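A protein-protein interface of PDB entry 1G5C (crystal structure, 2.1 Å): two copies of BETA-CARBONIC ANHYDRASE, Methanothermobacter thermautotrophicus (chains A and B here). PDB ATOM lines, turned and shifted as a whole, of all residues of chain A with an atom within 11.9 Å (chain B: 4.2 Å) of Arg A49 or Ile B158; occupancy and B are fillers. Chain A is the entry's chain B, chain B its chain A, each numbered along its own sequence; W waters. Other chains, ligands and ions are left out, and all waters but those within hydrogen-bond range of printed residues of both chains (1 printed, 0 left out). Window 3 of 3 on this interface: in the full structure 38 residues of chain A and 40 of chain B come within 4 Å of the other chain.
O of Ser B35 is in hydrogen-bond range of N of Gly A50, 2.8 Å away.
NE of Arg A49 is in hydrogen-bond range of O of Arg B36 (2.9 Å).
The guanidinium group (NH2) of Arg A49 lies within hydrogen-bond range of the backbone carbonyl oxygen (O) of Ile B158 (2.9 Å).
Water W1 lies within hydrogen-bond range of the guanidinium group (NH2) of Arg A49 and the side-chain amide oxygen (OD1) of Asn B159.
Of the printed residues of chain B, Pro A25 touches Ser B35.
Arg A49 touches just these residues of chain B: Ser B35, Arg B36, Ile B38, Leu B40 and Ile B158.
Of the printed residues of chain B, Gly A50 touches Ser B35 (2.8 Å).
Of the printed residues of chain B, Ala A52 touches Ser B35 (2.9 Å) and Ile B38 (3.2 Å).
Of the printed residues of chain B, Val A54 touches Ile B38.
Of chain A, only Pro A25, Arg A49, Gly A50 and Ala A52 come within 4 Å of Ser B35.
Arg B36 touches just one residue of chain A: Arg A49.
No residue of chain A comes within 4 Å of Leu B37.
Of chain A, only Glu A42, Gly A48, Arg A49, Ala A52 and Val A54 come within 4 Å of Ile B38.
Of chain A, only Arg A49 comes within 4 Å of Leu B40.
No residue of chain A comes within 4 Å of His B87.
No residue of chain A comes within 4 Å of Asp B89.
No residue of chain A comes within 4 Å of Ile B156.
No residue of chain A comes within 4 Å of Asp B157.
Ile B158 touches just one residue of chain A: Arg A49.
No residue of chain A comes within 4 Å of Asn B159.
The nearest printed residue of chain B that does not touch Arg A49 is Asn B159 (4.3 Å).
The nearest residue of chain A that does not touch Ile B158 is Gly A50 (8.8 Å).
No position is printed for both chains.
Of the 12 pairs that touch across the chains among the printed residues, none has its exchanged pair printed and touching as well.
Of the 20 printed residues of chain A, 7 touch a printed residue of chain B.
Hydrophobic or aromatic side chains of chain B that line the printed part of chain A: Ile B38 and Leu B40.
Among the printed residues, 12 pairs touch across the chains.
The side-chain carboxylate of Asp B89 is in salt-bridge range of the guanidinium group of Arg B36, at 2.9 Å.
The side-chain hydroxyl (OG1) of Thr B88 is in hydrogen-bond range of the backbone NH (N) of Ile B158 (2.9 Å).
NZ of Lys A53 sits at hydrogen-bond distance from O of Pro A25, at 3.0 Å.
N of Asp A39 is in hydrogen-bond range of OE1 of Glu A42.
The backbone NH of Ile A47 sits at hydrogen-bond distance from the backbone carbonyl oxygen of Glu A42 (2.8 Å).
The backbone NH (N) of Gly A48 sits at hydrogen-bond distance from the side-chain carboxylate (OD2) of Asp A51, 2.8 Å away.
Pro A25 touches Ser B35 (CG to OG, 3.4 Å).
Glu A42 touches Ile B38.
CG2 of Ile B38 touches C of Gly A48, 3.8 Å away.
O of Ser B35 touches C of Arg A49, 3.7 Å away.
O of Ile B38 touches CB of Arg A49 (3.3 Å).
NE of Arg A49 touches CD2 of Leu B40, at 3.6 Å.
CB of Ser B35 touches O of Ala A52, at 2.9 Å.
Ala A52 touches Ile B38 (O to CD1, 3.2 Å).
Val A54 touches Ile B38 (CG2 to CD1, 3.8 Å).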
ATOM      1  N   SER A  24       6.357 -30.999 -36.538  1.00  0.00           N
ATOM      2  CA  SER A  24       7.692 -31.575 -36.184  1.00  0.00           C
ATOM      3  C   SER A  24       7.712 -32.445 -34.930  1.00  0.00           C
ATOM      4  O   SER A  24       8.182 -33.580 -34.977  1.00  0.00           O
ATOM      5  CB  SER A  24       8.739 -30.464 -36.051  1.00  0.00           C
ATOM      6  OG  SER A  24       9.495 -30.358 -37.247  1.00  0.00           O
ATOM      7  N   PRO A  25       7.197 -31.935 -33.798  1.00  0.00           N
ATOM      8  CA  PRO A  25       7.192 -32.724 -32.555  1.00  0.00           C
ATOM      9  C   PRO A  25       6.603 -34.108 -32.825  1.00  0.00           C
ATOM     10  O   PRO A  25       5.624 -34.226 -33.557  1.00  0.00           O
ATOM     11  CB  PRO A  25       6.315 -31.889 -31.615  1.00  0.00           C
ATOM     12  CG  PRO A  25       6.434 -30.501 -32.149  1.00  0.00           C
ATOM     13  CD  PRO A  25       6.398 -30.710 -33.638  1.00  0.00           C
ATOM     14  N   LYS A  26       7.196 -35.148 -32.243  1.00  0.00           N
ATOM     15  CA  LYS A  26       6.732 -36.499 -32.453  1.00  0.00           C
ATOM     16  C   LYS A  26       5.658 -36.854 -31.430  1.00  0.00           C
ATOM     17  O   LYS A  26       4.982 -37.876 -31.571  1.00  0.00           O
ATOM     18  CB  LYS A  26       7.863 -37.523 -32.383  1.00  0.00           C
ATOM     19  CG  LYS A  26       8.480 -37.865 -33.741  1.00  0.00           C
ATOM     20  CD  LYS A  26       8.905 -36.624 -34.520  1.00  0.00           C
ATOM     21  CE  LYS A  26       9.752 -36.996 -35.747  1.00  0.00           C
ATOM     22  NZ  LYS A  26      11.133 -37.430 -35.369  1.00  0.00           N
ATOM     23  N   LEU A  27       5.485 -35.995 -30.423  1.00  0.00           N
ATOM     24  CA  LEU A  27       4.545 -36.232 -29.324  1.00  0.00           C
ATOM     25  C   LEU A  27       3.222 -35.481 -29.388  1.00  0.00           C
ATOM     26  O   LEU A  27       3.160 -34.352 -29.872  1.00  0.00           O
ATOM     27  CB  LEU A  27       5.235 -35.872 -28.004  1.00  0.00           C
ATOM     28  CG  LEU A  27       4.461 -35.973 -26.686  1.00  0.00           C
ATOM     29  CD1 LEU A  27       4.218 -37.449 -26.350  1.00  0.00           C
ATOM     30  CD2 LEU A  27       5.259 -35.302 -25.574  1.00  0.00           C
ATOM     31  N   ILE A  29      -0.060 -34.783 -26.667  1.00  0.00           N
ATOM     32  CA  ILE A  29      -0.582 -34.930 -25.319  1.00  0.00           C
ATOM     33  C   ILE A  29      -2.075 -34.648 -25.389  1.00  0.00           C
ATOM     34  O   ILE A  29      -2.497 -33.707 -26.067  1.00  0.00           O
ATOM     35  CB  ILE A  29       0.061 -33.915 -24.355  1.00  0.00           C
ATOM     36  CG1 ILE A  29       1.560 -34.198 -24.221  1.00  0.00           C
ATOM     37  CG2 ILE A  29      -0.617 -33.968 -22.993  1.00  0.00           C
ATOM     38  CD1 ILE A  29       2.300 -33.018 -23.680  1.00  0.00           C
ATOM     39  N   ASP A  39       0.469 -24.022 -17.370  1.00  0.00           N
ATOM     40  CA  ASP A  39       1.837 -23.842 -16.876  1.00  0.00           C
ATOM     41  C   ASP A  39       2.333 -25.003 -16.006  1.00  0.00           C
ATOM     42  O   ASP A  39       3.463 -25.465 -16.164  1.00  0.00           O
ATOM     43  CB  ASP A  39       1.976 -22.521 -16.141  1.00  0.00           C
ATOM     44  CG  ASP A  39       1.830 -21.337 -17.082  1.00  0.00           C
ATOM     45  OD1 ASP A  39       2.234 -21.482 -18.251  1.00  0.00           O
ATOM     46  OD2 ASP A  39       1.330 -20.285 -16.661  1.00  0.00           O
ATOM     47  N   LEU A  41       1.407 -28.165 -16.084  1.00  0.00           N
ATOM     48  CA  LEU A  41       1.659 -29.343 -16.903  1.00  0.00           C
ATOM     49  C   LEU A  41       2.961 -29.222 -17.711  1.00  0.00           C
ATOM     50  O   LEU A  41       3.719 -30.191 -17.840  1.00  0.00           O
ATOM     51  CB  LEU A  41       0.465 -29.598 -17.838  1.00  0.00           C
ATOM     52  CG  LEU A  41       0.432 -30.941 -18.572  1.00  0.00           C
ATOM     53  CD1 LEU A  41       0.498 -32.086 -17.558  1.00  0.00           C
ATOM     54  CD2 LEU A  41      -0.842 -31.033 -19.418  1.00  0.00           C
ATOM     55  N   GLU A  42       3.211 -28.034 -18.252  1.00  0.00           N
ATOM     56  CA  GLU A  42       4.422 -27.772 -19.022  1.00  0.00           C
ATOM     57  C   GLU A  42       5.685 -28.016 -18.183  1.00  0.00           C
ATOM     58  O   GLU A  42       6.611 -28.686 -18.641  1.00  0.00           O
ATOM     59  CB  GLU A  42       4.454 -26.325 -19.526  1.00  0.00           C
ATOM     60  CG  GLU A  42       3.436 -25.967 -20.617  1.00  0.00           C
ATOM     61  CD  GLU A  42       1.998 -26.055 -20.138  1.00  0.00           C
ATOM     62  OE1 GLU A  42       1.732 -25.778 -18.952  1.00  0.00           O
ATOM     63  OE2 GLU A  42       1.121 -26.396 -20.953  1.00  0.00           O
ATOM     64  N   ARG A  43       5.731 -27.458 -16.973  1.00  0.00           N
ATOM     65  CA  ARG A  43       6.900 -27.637 -16.106  1.00  0.00           C
ATOM     66  C   ARG A  43       6.994 -29.080 -15.620  1.00  0.00           C
ATOM     67  O   ARG A  43       8.081 -29.654 -15.568  1.00  0.00           O
ATOM     68  CB  ARG A  43       6.829 -26.702 -14.896  1.00  0.00           C
ATOM     69  CG  ARG A  43       7.115 -25.246 -15.221  1.00  0.00           C
ATOM     70  CD  ARG A  43       8.535 -25.087 -15.753  1.00  0.00           C
ATOM     71  NE  ARG A  43       8.892 -23.693 -15.991  1.00  0.00           N
ATOM     72  CZ  ARG A  43       8.826 -22.732 -15.073  1.00  0.00           C
ATOM     73  NH1 ARG A  43       8.407 -23.008 -13.841  1.00  0.00           N
ATOM     74  NH2 ARG A  43       9.185 -21.494 -15.386  1.00  0.00           N
ATOM     75  N   ALA A  44       5.850 -29.668 -15.273  1.00  0.00           N
ATOM     76  CA  ALA A  44       5.826 -31.036 -14.782  1.00  0.00           C
ATOM     77  C   ALA A  44       6.331 -32.057 -15.799  1.00  0.00           C
ATOM     78  O   ALA A  44       7.016 -33.009 -15.440  1.00  0.00           O
ATOM     79  CB  ALA A  44       4.412 -31.404 -14.319  1.00  0.00           C
ATOM     80  N   LEU A  45       6.001 -31.868 -17.068  1.00  0.00           N
ATOM     81  CA  LEU A  45       6.431 -32.804 -18.102  1.00  0.00           C
ATOM     82  C   LEU A  45       7.732 -32.397 -18.775  1.00  0.00           C
ATOM     83  O   LEU A  45       8.312 -33.178 -19.529  1.00  0.00           O
ATOM     84  CB  LEU A  45       5.357 -32.926 -19.183  1.00  0.00           C
ATOM     85  CG  LEU A  45       3.956 -33.377 -18.777  1.00  0.00           C
ATOM     86  CD1 LEU A  45       3.035 -33.263 -19.997  1.00  0.00           C
ATOM     87  CD2 LEU A  45       3.988 -34.798 -18.245  1.00  0.00           C
ATOM     88  N   GLY A  46       8.190 -31.182 -18.503  1.00  0.00           N
ATOM     89  CA  GLY A  46       9.388 -30.698 -19.162  1.00  0.00           C
ATOM     90  C   GLY A  46       9.048 -30.387 -20.615  1.00  0.00           C
ATOM     91  O   GLY A  46       9.876 -30.512 -21.500  1.00  0.00           O
ATOM     92  N   ILE A  47       7.807 -29.988 -20.865  1.00  0.00           N
ATOM     93  CA  ILE A  47       7.364 -29.672 -22.218  1.00  0.00           C
ATOM     94  C   ILE A  47       7.156 -28.162 -22.415  1.00  0.00           C
ATOM     95  O   ILE A  47       6.520 -27.500 -21.584  1.00  0.00           O
ATOM     96  CB  ILE A  47       6.069 -30.436 -22.520  1.00  0.00           C
ATOM     97  CG1 ILE A  47       6.394 -31.925 -22.624  1.00  0.00           C
ATOM     98  CG2 ILE A  47       5.408 -29.913 -23.800  1.00  0.00           C
ATOM     99  CD1 ILE A  47       5.197 -32.800 -22.744  1.00  0.00           C
ATOM    100  N   GLY A  48       7.713 -27.622 -23.497  1.00  0.00           N
ATOM    101  CA  GLY A  48       7.588 -26.200 -23.780  1.00  0.00           C
ATOM    102  C   GLY A  48       7.177 -25.944 -25.219  1.00  0.00           C
ATOM    103  O   GLY A  48       6.803 -26.868 -25.934  1.00  0.00           O
ATOM    104  N   ARG A  49       7.260 -24.690 -25.651  1.00  0.00           N
ATOM    105  CA  ARG A  49       6.862 -24.332 -27.002  1.00  0.00           C
ATOM    106  C   ARG A  49       7.518 -25.219 -28.047  1.00  0.00           C
ATOM    107  O   ARG A  49       8.737 -25.394 -28.052  1.00  0.00           O
ATOM    108  CB  ARG A  49       7.210 -22.871 -27.289  1.00  0.00           C
ATOM    109  CG  ARG A  49       6.728 -22.385 -28.648  1.00  0.00           C
ATOM    110  CD  ARG A  49       6.742 -20.844 -28.735  1.00  0.00           C
ATOM    111  NE  ARG A  49       6.179 -20.364 -30.001  1.00  0.00           N
ATOM    112  CZ  ARG A  49       6.887 -20.072 -31.085  1.00  0.00           C
ATOM    113  NH1 ARG A  49       8.215 -20.201 -31.077  1.00  0.00           N
ATOM    114  NH2 ARG A  49       6.265 -19.647 -32.176  1.00  0.00           N
ATOM    115  N   GLY A  50       6.696 -25.780 -28.925  1.00  0.00           N
ATOM    116  CA  GLY A  50       7.195 -26.632 -29.988  1.00  0.00           C
ATOM    117  C   GLY A  50       7.488 -28.076 -29.619  1.00  0.00           C
ATOM    118  O   GLY A  50       7.936 -28.827 -30.473  1.00  0.00           O
ATOM    119  N   ASP A  51       7.219 -28.490 -28.379  1.00  0.00           N
ATOM    120  CA  ASP A  51       7.522 -29.870 -27.976  1.00  0.00           C
ATOM    121  C   ASP A  51       6.407 -30.889 -28.166  1.00  0.00           C
ATOM    122  O   ASP A  51       6.641 -32.100 -28.040  1.00  0.00           O
ATOM    123  CB  ASP A  51       7.981 -29.926 -26.517  1.00  0.00           C
ATOM    124  CG  ASP A  51       9.313 -29.246 -26.304  1.00  0.00           C
ATOM    125  OD1 ASP A  51      10.095 -29.206 -27.266  1.00  0.00           O
ATOM    126  OD2 ASP A  51       9.581 -28.761 -25.179  1.00  0.00           O
ATOM    127  N   ALA A  52       5.202 -30.431 -28.477  1.00  0.00           N
ATOM    128  CA  ALA A  52       4.118 -31.378 -28.648  1.00  0.00           C
ATOM    129  C   ALA A  52       2.850 -30.756 -29.161  1.00  0.00           C
ATOM    130  O   ALA A  52       2.641 -29.563 -29.017  1.00  0.00           O
ATOM    131  CB  ALA A  52       3.821 -32.057 -27.299  1.00  0.00           C
ATOM    132  N   LYS A  53       2.013 -31.580 -29.781  1.00  0.00           N
ATOM    133  CA  LYS A  53       0.700 -31.130 -30.198  1.00  0.00           C
ATOM    134  C   LYS A  53      -0.121 -31.357 -28.937  1.00  0.00           C
ATOM    135  O   LYS A  53       0.088 -32.359 -28.235  1.00  0.00           O
ATOM    136  CB  LYS A  53       0.104 -32.010 -31.295  1.00  0.00           C
ATOM    137  CG  LYS A  53       0.533 -31.628 -32.666  1.00  0.00           C
ATOM    138  CD  LYS A  53       1.923 -32.139 -32.975  1.00  0.00           C
ATOM    139  CE  LYS A  53       2.093 -32.171 -34.471  1.00  0.00           C
ATOM    140  NZ  LYS A  53       3.496 -32.527 -34.838  1.00  0.00           N
ATOM    141  N   VAL A  54      -1.055 -30.457 -28.640  1.00  0.00           N
ATOM    142  CA  VAL A  54      -1.856 -30.623 -27.440  1.00  0.00           C
ATOM    143  C   VAL A  54      -3.352 -30.576 -27.697  1.00  0.00           C
ATOM    144  O   VAL A  54      -3.864 -29.599 -28.234  1.00  0.00           O
ATOM    145  CB  VAL A  54      -1.519 -29.552 -26.397  1.00  0.00           C
ATOM    146  CG1 VAL A  54      -2.383 -29.760 -25.151  1.00  0.00           C
ATOM    147  CG2 VAL A  54      -0.018 -29.609 -26.062  1.00  0.00           C
ATOM    148  N   SER B  35       1.856 -26.978 -31.742  1.00  0.00           N
ATOM    149  CA  SER B  35       2.887 -26.875 -30.698  1.00  0.00           C
ATOM    150  C   SER B  35       3.479 -25.492 -30.494  1.00  0.00           C
ATOM    151  O   SER B  35       4.038 -25.209 -29.425  1.00  0.00           O
ATOM    152  CB  SER B  35       4.036 -27.868 -30.948  1.00  0.00           C
ATOM    153  OG  SER B  35       4.852 -27.451 -32.029  1.00  0.00           O
ATOM    154  N   ARG B  36       3.354 -24.619 -31.492  1.00  0.00           N
ATOM    155  CA  ARG B  36       3.904 -23.274 -31.358  1.00  0.00           C
ATOM    156  C   ARG B  36       3.055 -22.358 -30.481  1.00  0.00           C
ATOM    157  O   ARG B  36       3.469 -21.234 -30.150  1.00  0.00           O
ATOM    158  CB  ARG B  36       4.086 -22.652 -32.743  1.00  0.00           C
ATOM    159  CG  ARG B  36       5.104 -23.398 -33.579  1.00  0.00           C
ATOM    160  CD  ARG B  36       5.056 -22.927 -35.000  1.00  0.00           C
ATOM    161  NE  ARG B  36       3.868 -23.444 -35.667  1.00  0.00           N
ATOM    162  CZ  ARG B  36       3.538 -23.160 -36.921  1.00  0.00           C
ATOM    163  NH1 ARG B  36       4.299 -22.351 -37.667  1.00  0.00           N
ATOM    164  NH2 ARG B  36       2.451 -23.709 -37.434  1.00  0.00           N
ATOM    165  N   LEU B  37       1.868 -22.828 -30.114  1.00  0.00           N
ATOM    166  CA  LEU B  37       0.989 -22.039 -29.254  1.00  0.00           C
ATOM    167  C   LEU B  37       1.306 -22.289 -27.785  1.00  0.00           C
ATOM    168  O   LEU B  37       0.893 -21.519 -26.916  1.00  0.00           O
ATOM    169  CB  LEU B  37      -0.480 -22.387 -29.518  1.00  0.00           C
ATOM    170  CG  LEU B  37      -1.013 -21.900 -30.868  1.00  0.00           C
ATOM    171  CD1 LEU B  37      -2.367 -22.532 -31.185  1.00  0.00           C
ATOM    172  CD2 LEU B  37      -1.111 -20.372 -30.827  1.00  0.00           C
ATOM    173  N   ILE B  38       2.019 -23.371 -27.495  1.00  0.00           N
ATOM    174  CA  ILE B  38       2.360 -23.664 -26.102  1.00  0.00           C
ATOM    175  C   ILE B  38       3.228 -22.514 -25.598  1.00  0.00           C
ATOM    176  O   ILE B  38       4.132 -22.066 -26.310  1.00  0.00           O
ATOM    177  CB  ILE B  38       3.151 -24.994 -25.973  1.00  0.00           C
ATOM    178  CG1 ILE B  38       2.296 -26.161 -26.482  1.00  0.00           C
ATOM    179  CG2 ILE B  38       3.528 -25.246 -24.497  1.00  0.00           C
ATOM    180  CD1 ILE B  38       3.067 -27.493 -26.569  1.00  0.00           C
ATOM    181  N   LEU B  40       3.630 -19.473 -25.706  1.00  0.00           N
ATOM    182  CA  LEU B  40       3.383 -18.225 -26.425  1.00  0.00           C
ATOM    183  C   LEU B  40       1.945 -17.698 -26.275  1.00  0.00           C
ATOM    184  O   LEU B  40       1.732 -16.509 -26.006  1.00  0.00           O
ATOM    185  CB  LEU B  40       3.699 -18.409 -27.909  1.00  0.00           C
ATOM    186  CG  LEU B  40       3.475 -17.218 -28.852  1.00  0.00           C
ATOM    187  CD1 LEU B  40       4.248 -15.985 -28.373  1.00  0.00           C
ATOM    188  CD2 LEU B  40       3.947 -17.602 -30.233  1.00  0.00           C
ATOM    189  N   HIS B  87      -4.848 -19.252 -35.541  1.00  0.00           N
ATOM    190  CA  HIS B  87      -3.493 -18.737 -35.675  1.00  0.00           C
ATOM    191  C   HIS B  87      -3.036 -18.840 -37.116  1.00  0.00           C
ATOM    192  O   HIS B  87      -3.531 -19.668 -37.871  1.00  0.00           O
ATOM    193  CB  HIS B  87      -2.522 -19.520 -34.778  1.00  0.00           C
ATOM    194  CG  HIS B  87      -2.356 -20.948 -35.187  1.00  0.00           C
ATOM    195  ND1 HIS B  87      -1.357 -21.362 -36.050  1.00  0.00           N
ATOM    196  CD2 HIS B  87      -3.082 -22.048 -34.898  1.00  0.00           C
ATOM    197  CE1 HIS B  87      -1.488 -22.654 -36.273  1.00  0.00           C
ATOM    198  NE2 HIS B  87      -2.523 -23.106 -35.587  1.00  0.00           N
ATOM    199  N   THR B  88      -2.080 -17.998 -37.485  1.00  0.00           N
ATOM    200  CA  THR B  88      -1.558 -18.012 -38.844  1.00  0.00           C
ATOM    201  C   THR B  88      -0.729 -19.275 -39.034  1.00  0.00           C
ATOM    202  O   THR B  88      -0.195 -19.840 -38.066  1.00  0.00           O
ATOM    203  CB  THR B  88      -0.655 -16.800 -39.106  1.00  0.00           C
ATOM    204  OG1 THR B  88       0.380 -16.771 -38.121  1.00  0.00           O
ATOM    205  CG2 THR B  88      -1.442 -15.501 -39.028  1.00  0.00           C
ATOM    206  N   ASP B  89      -0.617 -19.702 -40.284  1.00  0.00           N
ATOM    207  CA  ASP B  89       0.135 -20.896 -40.665  1.00  0.00           C
ATOM    208  C   ASP B  89      -0.385 -22.151 -39.969  1.00  0.00           C
ATOM    209  O   ASP B  89       0.394 -22.945 -39.428  1.00  0.00           O
ATOM    210  CB  ASP B  89       1.631 -20.712 -40.377  1.00  0.00           C
ATOM    211  CG  ASP B  89       2.480 -21.811 -40.999  1.00  0.00           C
ATOM    212  OD1 ASP B  89       2.123 -22.278 -42.086  1.00  0.00           O
ATOM    213  OD2 ASP B  89       3.507 -22.206 -40.418  1.00  0.00           O
ATOM    214  N   ILE B 156      -4.166 -15.199 -33.904  1.00  0.00           N
ATOM    215  CA  ILE B 156      -2.851 -14.797 -33.421  1.00  0.00           C
ATOM    216  C   ILE B 156      -1.751 -15.105 -34.444  1.00  0.00           C
ATOM    217  O   ILE B 156      -1.804 -16.129 -35.119  1.00  0.00           O
ATOM    218  CB  ILE B 156      -2.508 -15.527 -32.075  1.00  0.00           C
ATOM    219  CG1 ILE B 156      -1.231 -14.942 -31.469  1.00  0.00           C
ATOM    220  CG2 ILE B 156      -2.319 -17.046 -32.312  1.00  0.00           C
ATOM    221  CD1 ILE B 156      -0.941 -15.468 -30.033  1.00  0.00           C
ATOM    222  N   ASP B 157      -0.772 -14.206 -34.566  1.00  0.00           N
ATOM    223  CA  ASP B 157       0.373 -14.427 -35.455  1.00  0.00           C
ATOM    224  C   ASP B 157       1.194 -15.512 -34.750  1.00  0.00           C
ATOM    225  O   ASP B 157       1.680 -15.294 -33.642  1.00  0.00           O
ATOM    226  CB  ASP B 157       1.213 -13.149 -35.585  1.00  0.00           C
ATOM    227  CG  ASP B 157       2.398 -13.320 -36.533  1.00  0.00           C
ATOM    228  OD1 ASP B 157       3.247 -14.224 -36.306  1.00  0.00           O
ATOM    229  OD2 ASP B 157       2.483 -12.554 -37.513  1.00  0.00           O
ATOM    230  N   ILE B 158       1.368 -16.664 -35.389  1.00  0.00           N
ATOM    231  CA  ILE B 158       2.071 -17.768 -34.762  1.00  0.00           C
ATOM    232  C   ILE B 158       3.549 -17.523 -34.415  1.00  0.00           C
ATOM    233  O   ILE B 158       4.130 -18.229 -33.579  1.00  0.00           O
ATOM    234  CB  ILE B 158       1.904 -19.062 -35.618  1.00  0.00           C
ATOM    235  CG1 ILE B 158       2.239 -20.304 -34.774  1.00  0.00           C
ATOM    236  CG2 ILE B 158       2.778 -18.999 -36.880  1.00  0.00           C
ATOM    237  CD1 ILE B 158       1.338 -20.490 -33.542  1.00  0.00           C
ATOM    238  N   ASN B 159       4.158 -16.510 -35.014  1.00  0.00           N
ATOM    239  CA  ASN B 159       5.553 -16.234 -34.710  1.00  0.00           C
ATOM    240  C   ASN B 159       5.779 -15.089 -33.730  1.00  0.00           C
ATOM    241  O   ASN B 159       6.744 -15.108 -32.973  1.00  0.00           O
ATOM    242  CB  ASN B 159       6.320 -15.951 -36.004  1.00  0.00           C
ATOM    243  CG  ASN B 159       6.227 -17.099 -36.989  1.00  0.00           C
ATOM    244  OD1 ASN B 159       6.571 -18.235 -36.666  1.00  0.00           O
ATOM    245  ND2 ASN B 159       5.747 -16.812 -38.189  1.00  0.00           N
ATOM    246  N   THR B 160       4.887 -14.107 -33.726  1.00  0.00           N
ATOM    247  CA  THR B 160       5.048 -12.940 -32.867  1.00  0.00           C
ATOM    248  C   THR B 160       4.103 -12.878 -31.654  1.00  0.00           C
ATOM    249  O   THR B 160       4.404 -12.197 -30.674  1.00  0.00           O
ATOM    250  CB  THR B 160       4.858 -11.644 -33.690  1.00  0.00           C
ATOM    251  OG1 THR B 160       3.463 -11.470 -33.984  1.00  0.00           O
ATOM    252  CG2 THR B 160       5.638 -11.723 -35.030  1.00  0.00           C
HETATM  253  O   HOH W   1       7.925 -19.016 -34.331  1.00  0.00           O
